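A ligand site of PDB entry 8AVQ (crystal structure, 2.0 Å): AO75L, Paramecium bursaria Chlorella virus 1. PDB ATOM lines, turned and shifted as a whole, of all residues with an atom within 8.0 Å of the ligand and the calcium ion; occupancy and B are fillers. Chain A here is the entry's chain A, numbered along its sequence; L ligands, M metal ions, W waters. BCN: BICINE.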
ATOM      1  N   ARG A 163     -11.835  20.234 -34.783  1.00  0.00           N
ATOM      2  CA  ARG A 163     -10.451  20.503 -34.282  1.00  0.00           C
ATOM      3  C   ARG A 163     -10.292  19.952 -32.866  1.00  0.00           C
ATOM      4  O   ARG A 163      -9.242  19.363 -32.588  1.00  0.00           O
ATOM      5  CB  ARG A 163     -10.139  22.004 -34.314  1.00  0.00           C
ATOM      6  CG  ARG A 163     -10.092  22.577 -35.717  1.00  0.00           C
ATOM      7  CD  ARG A 163      -9.090  23.703 -35.828  1.00  0.00           C
ATOM      8  NE  ARG A 163      -7.718  23.224 -35.675  1.00  0.00           N
ATOM      9  CZ  ARG A 163      -6.683  23.993 -35.366  1.00  0.00           C
ATOM     10  NH1 ARG A 163      -6.864  25.287 -35.171  1.00  0.00           N
ATOM     11  NH2 ARG A 163      -5.473  23.473 -35.259  1.00  0.00           N
ATOM     12  N   LEU A 167      -7.700  16.947 -32.147  1.00  0.00           N
ATOM     13  CA  LEU A 167      -6.478  17.324 -31.387  1.00  0.00           C
ATOM     14  C   LEU A 167      -6.401  16.605 -30.032  1.00  0.00           C
ATOM     15  O   LEU A 167      -5.277  16.264 -29.603  1.00  0.00           O
ATOM     16  CB  LEU A 167      -6.432  18.839 -31.211  1.00  0.00           C
ATOM     17  CG  LEU A 167      -6.055  19.649 -32.460  1.00  0.00           C
ATOM     18  CD1 LEU A 167      -6.241  21.140 -32.205  1.00  0.00           C
ATOM     19  CD2 LEU A 167      -4.633  19.367 -32.904  1.00  0.00           C
ATOM     20  N   TYR A 168      -7.529  16.419 -29.342  1.00  0.00           N
ATOM     21  CA  TYR A 168      -7.522  16.168 -27.871  1.00  0.00           C
ATOM     22  C   TYR A 168      -8.166  14.831 -27.484  1.00  0.00           C
ATOM     23  O   TYR A 168      -8.076  14.504 -26.281  1.00  0.00           O
ATOM     24  CB  TYR A 168      -8.161  17.346 -27.149  1.00  0.00           C
ATOM     25  CG  TYR A 168      -7.503  18.667 -27.462  1.00  0.00           C
ATOM     26  CD1 TYR A 168      -6.154  18.862 -27.211  1.00  0.00           C
ATOM     27  CD2 TYR A 168      -8.206  19.702 -28.032  1.00  0.00           C
ATOM     28  CE1 TYR A 168      -5.527  20.052 -27.515  1.00  0.00           C
ATOM     29  CE2 TYR A 168      -7.599  20.902 -28.341  1.00  0.00           C
ATOM     30  CZ  TYR A 168      -6.255  21.082 -28.083  1.00  0.00           C
ATOM     31  OH  TYR A 168      -5.649  22.274 -28.380  1.00  0.00           O
ATOM     32  N   PHE A 200     -14.924  21.092 -22.610  1.00  0.00           N
ATOM     33  CA  PHE A 200     -14.960  21.793 -23.920  1.00  0.00           C
ATOM     34  C   PHE A 200     -16.402  22.246 -24.131  1.00  0.00           C
ATOM     35  O   PHE A 200     -17.282  21.371 -24.126  1.00  0.00           O
ATOM     36  CB  PHE A 200     -14.487  20.868 -25.043  1.00  0.00           C
ATOM     37  CG  PHE A 200     -13.023  20.518 -24.983  1.00  0.00           C
ATOM     38  CD1 PHE A 200     -12.063  21.428 -25.388  1.00  0.00           C
ATOM     39  CD2 PHE A 200     -12.611  19.269 -24.546  1.00  0.00           C
ATOM     40  CE1 PHE A 200     -10.718  21.100 -25.339  1.00  0.00           C
ATOM     41  CE2 PHE A 200     -11.275  18.938 -24.507  1.00  0.00           C
ATOM     42  CZ  PHE A 200     -10.317  19.864 -24.896  1.00  0.00           C
ATOM     43  N   ILE A 223     -14.649  25.781 -21.397  1.00  0.00           N
ATOM     44  CA  ILE A 223     -13.675  26.387 -22.351  1.00  0.00           C
ATOM     45  C   ILE A 223     -14.454  26.815 -23.607  1.00  0.00           C
ATOM     46  O   ILE A 223     -15.110  25.954 -24.213  1.00  0.00           O
ATOM     47  CB  ILE A 223     -12.518  25.419 -22.689  1.00  0.00           C
ATOM     48  CG1 ILE A 223     -11.869  24.850 -21.418  1.00  0.00           C
ATOM     49  CG2 ILE A 223     -11.484  26.092 -23.586  1.00  0.00           C
ATOM     50  CD1 ILE A 223     -10.946  23.676 -21.661  1.00  0.00           C
ATOM     51  N   VAL A 224     -14.391  28.101 -23.942  1.00  0.00           N
ATOM     52  CA  VAL A 224     -15.248  28.750 -24.983  1.00  0.00           C
ATOM     53  C   VAL A 224     -14.367  29.672 -25.824  1.00  0.00           C
ATOM     54  O   VAL A 224     -13.561  30.416 -25.227  1.00  0.00           O
ATOM     55  CB  VAL A 224     -16.400  29.532 -24.325  1.00  0.00           C
ATOM     56  CG1 VAL A 224     -17.305  30.192 -25.356  1.00  0.00           C
ATOM     57  CG2 VAL A 224     -17.220  28.650 -23.385  1.00  0.00           C
ATOM     58  N   LYS A 225     -14.511  29.640 -27.151  1.00  0.00           N
ATOM     59  CA  LYS A 225     -13.764  30.542 -28.064  1.00  0.00           C
ATOM     60  C   LYS A 225     -14.309  31.958 -27.891  1.00  0.00           C
ATOM     61  O   LYS A 225     -15.552  32.111 -27.818  1.00  0.00           O
ATOM     62  CB  LYS A 225     -13.851  30.054 -29.518  1.00  0.00           C
ATOM     63  CG  LYS A 225     -13.000  30.847 -30.508  1.00  0.00           C
ATOM     64  CD  LYS A 225     -12.768  30.114 -31.804  1.00  0.00           C
ATOM     65  CE  LYS A 225     -11.741  30.764 -32.700  1.00  0.00           C
ATOM     66  NZ  LYS A 225     -12.348  31.821 -33.544  1.00  0.00           N
ATOM     67  N   LYS A 226     -13.418  32.948 -27.792  1.00  0.00           N
ATOM     68  CA  LYS A 226     -13.776  34.386 -27.691  1.00  0.00           C
ATOM     69  C   LYS A 226     -14.729  34.753 -28.839  1.00  0.00           C
ATOM     70  O   LYS A 226     -14.476  34.335 -29.983  1.00  0.00           O
ATOM     71  CB  LYS A 226     -12.526  35.268 -27.744  1.00  0.00           C
ATOM     72  CG  LYS A 226     -11.679  35.242 -26.477  1.00  0.00           C
ATOM     73  CD  LYS A 226     -10.349  35.944 -26.654  1.00  0.00           C
ATOM     74  CE  LYS A 226      -9.424  35.745 -25.465  1.00  0.00           C
ATOM     75  NZ  LYS A 226      -8.158  36.481 -25.662  1.00  0.00           N
ATOM     76  N   LEU A 239     -13.211  29.993 -19.242  1.00  0.00           N
ATOM     77  CA  LEU A 239     -11.884  30.097 -19.889  1.00  0.00           C
ATOM     78  C   LEU A 239     -12.094  30.438 -21.356  1.00  0.00           C
ATOM     79  O   LEU A 239     -12.491  29.533 -22.122  1.00  0.00           O
ATOM     80  CB  LEU A 239     -11.100  28.800 -19.700  1.00  0.00           C
ATOM     81  CG  LEU A 239      -9.691  28.802 -20.307  1.00  0.00           C
ATOM     82  CD1 LEU A 239      -8.917  30.042 -19.905  1.00  0.00           C
ATOM     83  CD2 LEU A 239      -8.927  27.550 -19.910  1.00  0.00           C
ATOM     84  N   PHE A 240     -11.869  31.704 -21.725  1.00  0.00           N
ATOM     85  CA  PHE A 240     -12.019  32.229 -23.106  1.00  0.00           C
ATOM     86  C   PHE A 240     -10.694  32.045 -23.861  1.00  0.00           C
ATOM     87  O   PHE A 240      -9.641  32.496 -23.377  1.00  0.00           O
ATOM     88  CB  PHE A 240     -12.479  33.683 -23.092  1.00  0.00           C
ATOM     89  CG  PHE A 240     -13.940  33.822 -22.714  1.00  0.00           C
ATOM     90  CD1 PHE A 240     -14.927  33.304 -23.529  1.00  0.00           C
ATOM     91  CD2 PHE A 240     -14.311  34.460 -21.544  1.00  0.00           C
ATOM     92  CE1 PHE A 240     -16.261  33.429 -23.194  1.00  0.00           C
ATOM     93  CE2 PHE A 240     -15.649  34.598 -21.209  1.00  0.00           C
ATOM     94  CZ  PHE A 240     -16.622  34.076 -22.025  1.00  0.00           C
ATOM     95  N   VAL A 241     -10.758  31.383 -25.020  1.00  0.00           N
ATOM     96  CA  VAL A 241      -9.574  31.011 -25.832  1.00  0.00           C
ATOM     97  C   VAL A 241      -9.645  31.745 -27.176  1.00  0.00           C
ATOM     98  O   VAL A 241     -10.765  32.013 -27.666  1.00  0.00           O
ATOM     99  CB  VAL A 241      -9.463  29.475 -26.000  1.00  0.00           C
ATOM    100  CG1 VAL A 241      -9.255  28.803 -24.650  1.00  0.00           C
ATOM    101  CG2 VAL A 241     -10.669  28.871 -26.704  1.00  0.00           C
ATOM    102  N   ASN A 242      -8.478  32.112 -27.727  1.00  0.00           N
ATOM    103  CA  ASN A 242      -8.325  32.778 -29.042  1.00  0.00           C
ATOM    104  C   ASN A 242      -8.575  31.759 -30.166  1.00  0.00           C
ATOM    105  O   ASN A 242      -9.030  32.177 -31.244  1.00  0.00           O
ATOM    106  CB  ASN A 242      -6.940  33.392 -29.206  1.00  0.00           C
ATOM    107  CG  ASN A 242      -6.685  34.524 -28.221  1.00  0.00           C
ATOM    108  OD1 ASN A 242      -7.541  35.392 -28.055  1.00  0.00           O
ATOM    109  ND2 ASN A 242      -5.539  34.515 -27.571  1.00  0.00           N
ATOM    110  N   ASP A 243      -8.223  30.491 -29.915  1.00  0.00           N
ATOM    111  CA  ASP A 243      -8.350  29.361 -30.874  1.00  0.00           C
ATOM    112  C   ASP A 243      -8.322  28.053 -30.074  1.00  0.00           C
ATOM    113  O   ASP A 243      -8.258  28.129 -28.830  1.00  0.00           O
ATOM    114  CB  ASP A 243      -7.232  29.402 -31.927  1.00  0.00           C
ATOM    115  CG  ASP A 243      -5.835  29.306 -31.347  1.00  0.00           C
ATOM    116  OD1 ASP A 243      -5.624  28.490 -30.425  1.00  0.00           O
ATOM    117  OD2 ASP A 243      -4.958  30.049 -31.815  1.00  0.00           O
ATOM    118  N   TRP A 244      -8.357  26.911 -30.754  1.00  0.00           N
ATOM    119  CA  TRP A 244      -8.478  25.576 -30.122  1.00  0.00           C
ATOM    120  C   TRP A 244      -7.144  24.827 -30.163  1.00  0.00           C
ATOM    121  O   TRP A 244      -7.128  23.649 -29.785  1.00  0.00           O
ATOM    122  CB  TRP A 244      -9.620  24.807 -30.795  1.00  0.00           C
ATOM    123  CG  TRP A 244     -10.951  25.356 -30.409  1.00  0.00           C
ATOM    124  CD1 TRP A 244     -11.823  26.060 -31.185  1.00  0.00           C
ATOM    125  CD2 TRP A 244     -11.532  25.314 -29.096  1.00  0.00           C
ATOM    126  NE1 TRP A 244     -12.925  26.428 -30.464  1.00  0.00           N
ATOM    127  CE2 TRP A 244     -12.776  25.987 -29.173  1.00  0.00           C
ATOM    128  CE3 TRP A 244     -11.141  24.755 -27.879  1.00  0.00           C
ATOM    129  CZ2 TRP A 244     -13.625  26.099 -28.075  1.00  0.00           C
ATOM    130  CZ3 TRP A 244     -11.972  24.879 -26.788  1.00  0.00           C
ATOM    131  CH2 TRP A 244     -13.193  25.534 -26.890  1.00  0.00           C
ATOM    132  N   GLU A 245      -6.067  25.512 -30.565  1.00  0.00           N
ATOM    133  CA  GLU A 245      -4.726  24.890 -30.768  1.00  0.00           C
ATOM    134  C   GLU A 245      -3.851  25.140 -29.539  1.00  0.00           C
ATOM    135  O   GLU A 245      -3.902  26.258 -28.968  1.00  0.00           O
ATOM    136  CB  GLU A 245      -4.104  25.438 -32.045  1.00  0.00           C
ATOM    137  CG  GLU A 245      -2.905  24.636 -32.525  1.00  0.00           C
ATOM    138  CD  GLU A 245      -2.477  24.928 -33.957  1.00  0.00           C
ATOM    139  OE1 GLU A 245      -3.358  25.214 -34.787  1.00  0.00           O
ATOM    140  OE2 GLU A 245      -1.265  24.856 -34.235  1.00  0.00           O
ATOM    141  N   ASN A 246      -3.065  24.118 -29.167  1.00  0.00           N
ATOM    142  CA  ASN A 246      -1.995  24.183 -28.133  1.00  0.00           C
ATOM    143  C   ASN A 246      -2.605  24.275 -26.725  1.00  0.00           C
ATOM    144  O   ASN A 246      -1.958  24.887 -25.863  1.00  0.00           O
ATOM    145  CB  ASN A 246      -1.018  25.328 -28.394  1.00  0.00           C
ATOM    146  CG  ASN A 246      -0.298  25.170 -29.719  1.00  0.00           C
ATOM    147  OD1 ASN A 246      -0.204  26.114 -30.499  1.00  0.00           O
ATOM    148  ND2 ASN A 246       0.188  23.969 -29.985  1.00  0.00           N
ATOM    149  N   ILE A 247      -3.779  23.693 -26.506  1.00  0.00           N
ATOM    150  CA  ILE A 247      -4.277  23.397 -25.128  1.00  0.00           C
ATOM    151  C   ILE A 247      -3.406  22.240 -24.609  1.00  0.00           C
ATOM    152  O   ILE A 247      -3.385  21.184 -25.280  1.00  0.00           O
ATOM    153  CB  ILE A 247      -5.778  23.064 -25.090  1.00  0.00           C
ATOM    154  CG1 ILE A 247      -6.628  24.289 -25.457  1.00  0.00           C
ATOM    155  CG2 ILE A 247      -6.174  22.493 -23.740  1.00  0.00           C
ATOM    156  CD1 ILE A 247      -8.091  23.979 -25.683  1.00  0.00           C
ATOM    157  N   THR A 248      -2.703  22.473 -23.496  1.00  0.00           N
ATOM    158  CA  THR A 248      -1.848  21.478 -22.798  1.00  0.00           C
ATOM    159  C   THR A 248      -2.346  21.300 -21.373  1.00  0.00           C
ATOM    160  O   THR A 248      -3.088  22.170 -20.868  1.00  0.00           O
ATOM    161  CB  THR A 248      -0.368  21.893 -22.838  1.00  0.00           C
ATOM    162  OG1 THR A 248      -0.173  23.056 -22.042  1.00  0.00           O
ATOM    163  CG2 THR A 248       0.135  22.161 -24.233  1.00  0.00           C
ATOM    164  N   TYR A 251      -0.992  24.242 -19.391  1.00  0.00           N
ATOM    165  CA  TYR A 251      -1.863  25.413 -19.684  1.00  0.00           C
ATOM    166  C   TYR A 251      -3.115  25.371 -18.790  1.00  0.00           C
ATOM    167  O   TYR A 251      -3.416  26.381 -18.134  1.00  0.00           O
ATOM    168  CB  TYR A 251      -2.277  25.464 -21.154  1.00  0.00           C
ATOM    169  CG  TYR A 251      -3.334  26.503 -21.435  1.00  0.00           C
ATOM    170  CD1 TYR A 251      -3.018  27.845 -21.471  1.00  0.00           C
ATOM    171  CD2 TYR A 251      -4.657  26.134 -21.622  1.00  0.00           C
ATOM    172  CE1 TYR A 251      -3.975  28.814 -21.715  1.00  0.00           C
ATOM    173  CE2 TYR A 251      -5.635  27.084 -21.863  1.00  0.00           C
ATOM    174  CZ  TYR A 251      -5.290  28.425 -21.913  1.00  0.00           C
ATOM    175  OH  TYR A 251      -6.249  29.365 -22.149  1.00  0.00           O
ATOM    176  N   LEU A 252      -3.831  24.252 -18.779  1.00  0.00           N
ATOM    177  CA  LEU A 252      -5.122  24.109 -18.051  1.00  0.00           C
ATOM    178  C   LEU A 252      -4.882  24.111 -16.538  1.00  0.00           C
ATOM    179  O   LEU A 252      -5.691  24.717 -15.818  1.00  0.00           O
ATOM    180  CB  LEU A 252      -5.821  22.828 -18.485  1.00  0.00           C
ATOM    181  CG  LEU A 252      -6.397  22.849 -19.903  1.00  0.00           C
ATOM    182  CD1 LEU A 252      -7.026  21.508 -20.222  1.00  0.00           C
ATOM    183  CD2 LEU A 252      -7.418  23.965 -20.073  1.00  0.00           C
ATOM    184  N   GLN A 255      -4.433  27.741 -15.612  1.00  0.00           N
ATOM    185  CA  GLN A 255      -5.719  28.482 -15.737  1.00  0.00           C
ATOM    186  C   GLN A 255      -6.670  28.047 -14.618  1.00  0.00           C
ATOM    187  O   GLN A 255      -7.397  28.920 -14.125  1.00  0.00           O
ATOM    188  CB  GLN A 255      -6.334  28.291 -17.130  1.00  0.00           C
ATOM    189  CG  GLN A 255      -5.520  28.911 -18.254  1.00  0.00           C
ATOM    190  CD  GLN A 255      -5.341  30.407 -18.115  1.00  0.00           C
ATOM    191  OE1 GLN A 255      -6.269  31.126 -17.758  1.00  0.00           O
ATOM    192  NE2 GLN A 255      -4.143  30.884 -18.412  1.00  0.00           N
HETATM  193  N1  BCN L   1      -4.030  28.629 -25.902  1.00  0.00           N
HETATM  194  C1  BCN L   1      -4.455  29.993 -25.538  1.00  0.00           C
HETATM  195  C2  BCN L   1      -5.401  30.613 -26.565  1.00  0.00           C
HETATM  196  O21 BCN L   1      -6.132  31.540 -26.173  1.00  0.00           O
HETATM  197  O22 BCN L   1      -5.389  30.130 -27.713  1.00  0.00           O
HETATM  198  C3  BCN L   1      -2.643  28.335 -25.526  1.00  0.00           C
HETATM  199  C4  BCN L   1      -1.628  29.018 -26.412  1.00  0.00           C
HETATM  200  O4  BCN L   1      -1.875  28.742 -27.767  1.00  0.00           O
HETATM  201  C5  BCN L   1      -4.978  27.598 -25.451  1.00  0.00           C
HETATM  202  C6  BCN L   1      -6.300  27.627 -26.195  1.00  0.00           C
HETATM  203  O6  BCN L   1      -6.126  27.307 -27.564  1.00  0.00           O
HETATM  204 CA    CA M   1      -4.104  28.521 -28.597  1.00  0.00          CA
HETATM  205 MG    MG M   2       1.618  24.947 -22.877  1.00  0.00          MG
HETATM  206  O   HOH W   1      -2.538  28.267 -30.453  1.00  0.00           O
HETATM  207  O   HOH W   2      -6.789  32.935 -24.173  1.00  0.00           O
HETATM  208  O   HOH W   3      -2.969  32.650 -27.704  1.00  0.00           O
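The backbone NH of Asn 242 lies within hydrogen-bond range of an oxygen (O21) of the ligand (2.9 Å).
The backbone carbonyl oxygen (O) of Asp 243 lies close to an oxygen (O6) of the ligand, at 2.6 Å.
An oxygen (O21) of the ligand sits at hydrogen-bond distance from the side-chain amide nitrogen of Asn 242 (3.3 Å).
The backbone NH of Glu 245 lies close to an oxygen (O6) of the ligand (3.5 Å).
The guanidinium group (NH2) of Arg 163 is in salt-bridge range of the side-chain carboxylate (OE1) of Glu 245, 2.8 Å away.
The backbone carbonyl oxygen (O) of Val 224 sits at hydrogen-bond distance from the backbone NH (N) of Val 241 (3.0 Å).
OD1 of Asn 242 sits at hydrogen-bond distance from NZ of Lys 226, 2.7 Å away.
The side-chain hydroxyl of Thr 248 lies within hydrogen-bond range of the backbone NH of Tyr 251 (3.0 Å).
N of Asn 246 lies within hydrogen-bond range of OH of Tyr 168 (3.3 Å).
N of Ile 247 is in hydrogen-bond range of OH of Tyr 168, 3.0 Å away.
The backbone carbonyl oxygen of Trp 244 lies within hydrogen-bond range of the side-chain hydroxyl of Tyr 168, at 2.5 Å.
The backbone carbonyl oxygen of Val 241 sits at hydrogen-bond distance from the backbone NH of Lys 226 (2.8 Å).
Merely in contact with the ligand: Val 241 (3.5 Å), Trp 244 (3.7 Å), Asn 246 (3.5 Å), Ile 247 (3.4 Å) and Tyr 251 (3.6 Å).
Hydrophobic or aromatic side chains that line the ligand: Val 241, Ile 247 and Tyr 251.
The nearest printed residue that does not touch the calcium ion is Asn 246 (4.4 Å).
The calcium ion is bound by O22 of the ligand (2.2 Å).
The calcium ion is bound by O of Glu 245 (2.3 Å).
The calcium ion is bound by OD1 of Asp 243 (2.4 Å).
The calcium ion is bound by an oxygen (O4) of the ligand (2.4 Å).
Water W1 binds the calcium ion (2.4 Å).
O6 of the ligand binds the calcium ion.
The calcium ion is bound by N1 of the ligand (2.7 Å).
Water W1 lies within hydrogen-bond range of the side-chain amide oxygen (OD1) of Asn 246 (3.2 Å) and the side-chain carboxylate (OD2) of Asp 243 (3.3 Å).
Water W2 bridges an oxygen (O21) of the ligand and the backbone carbonyl oxygen of Phe 240.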
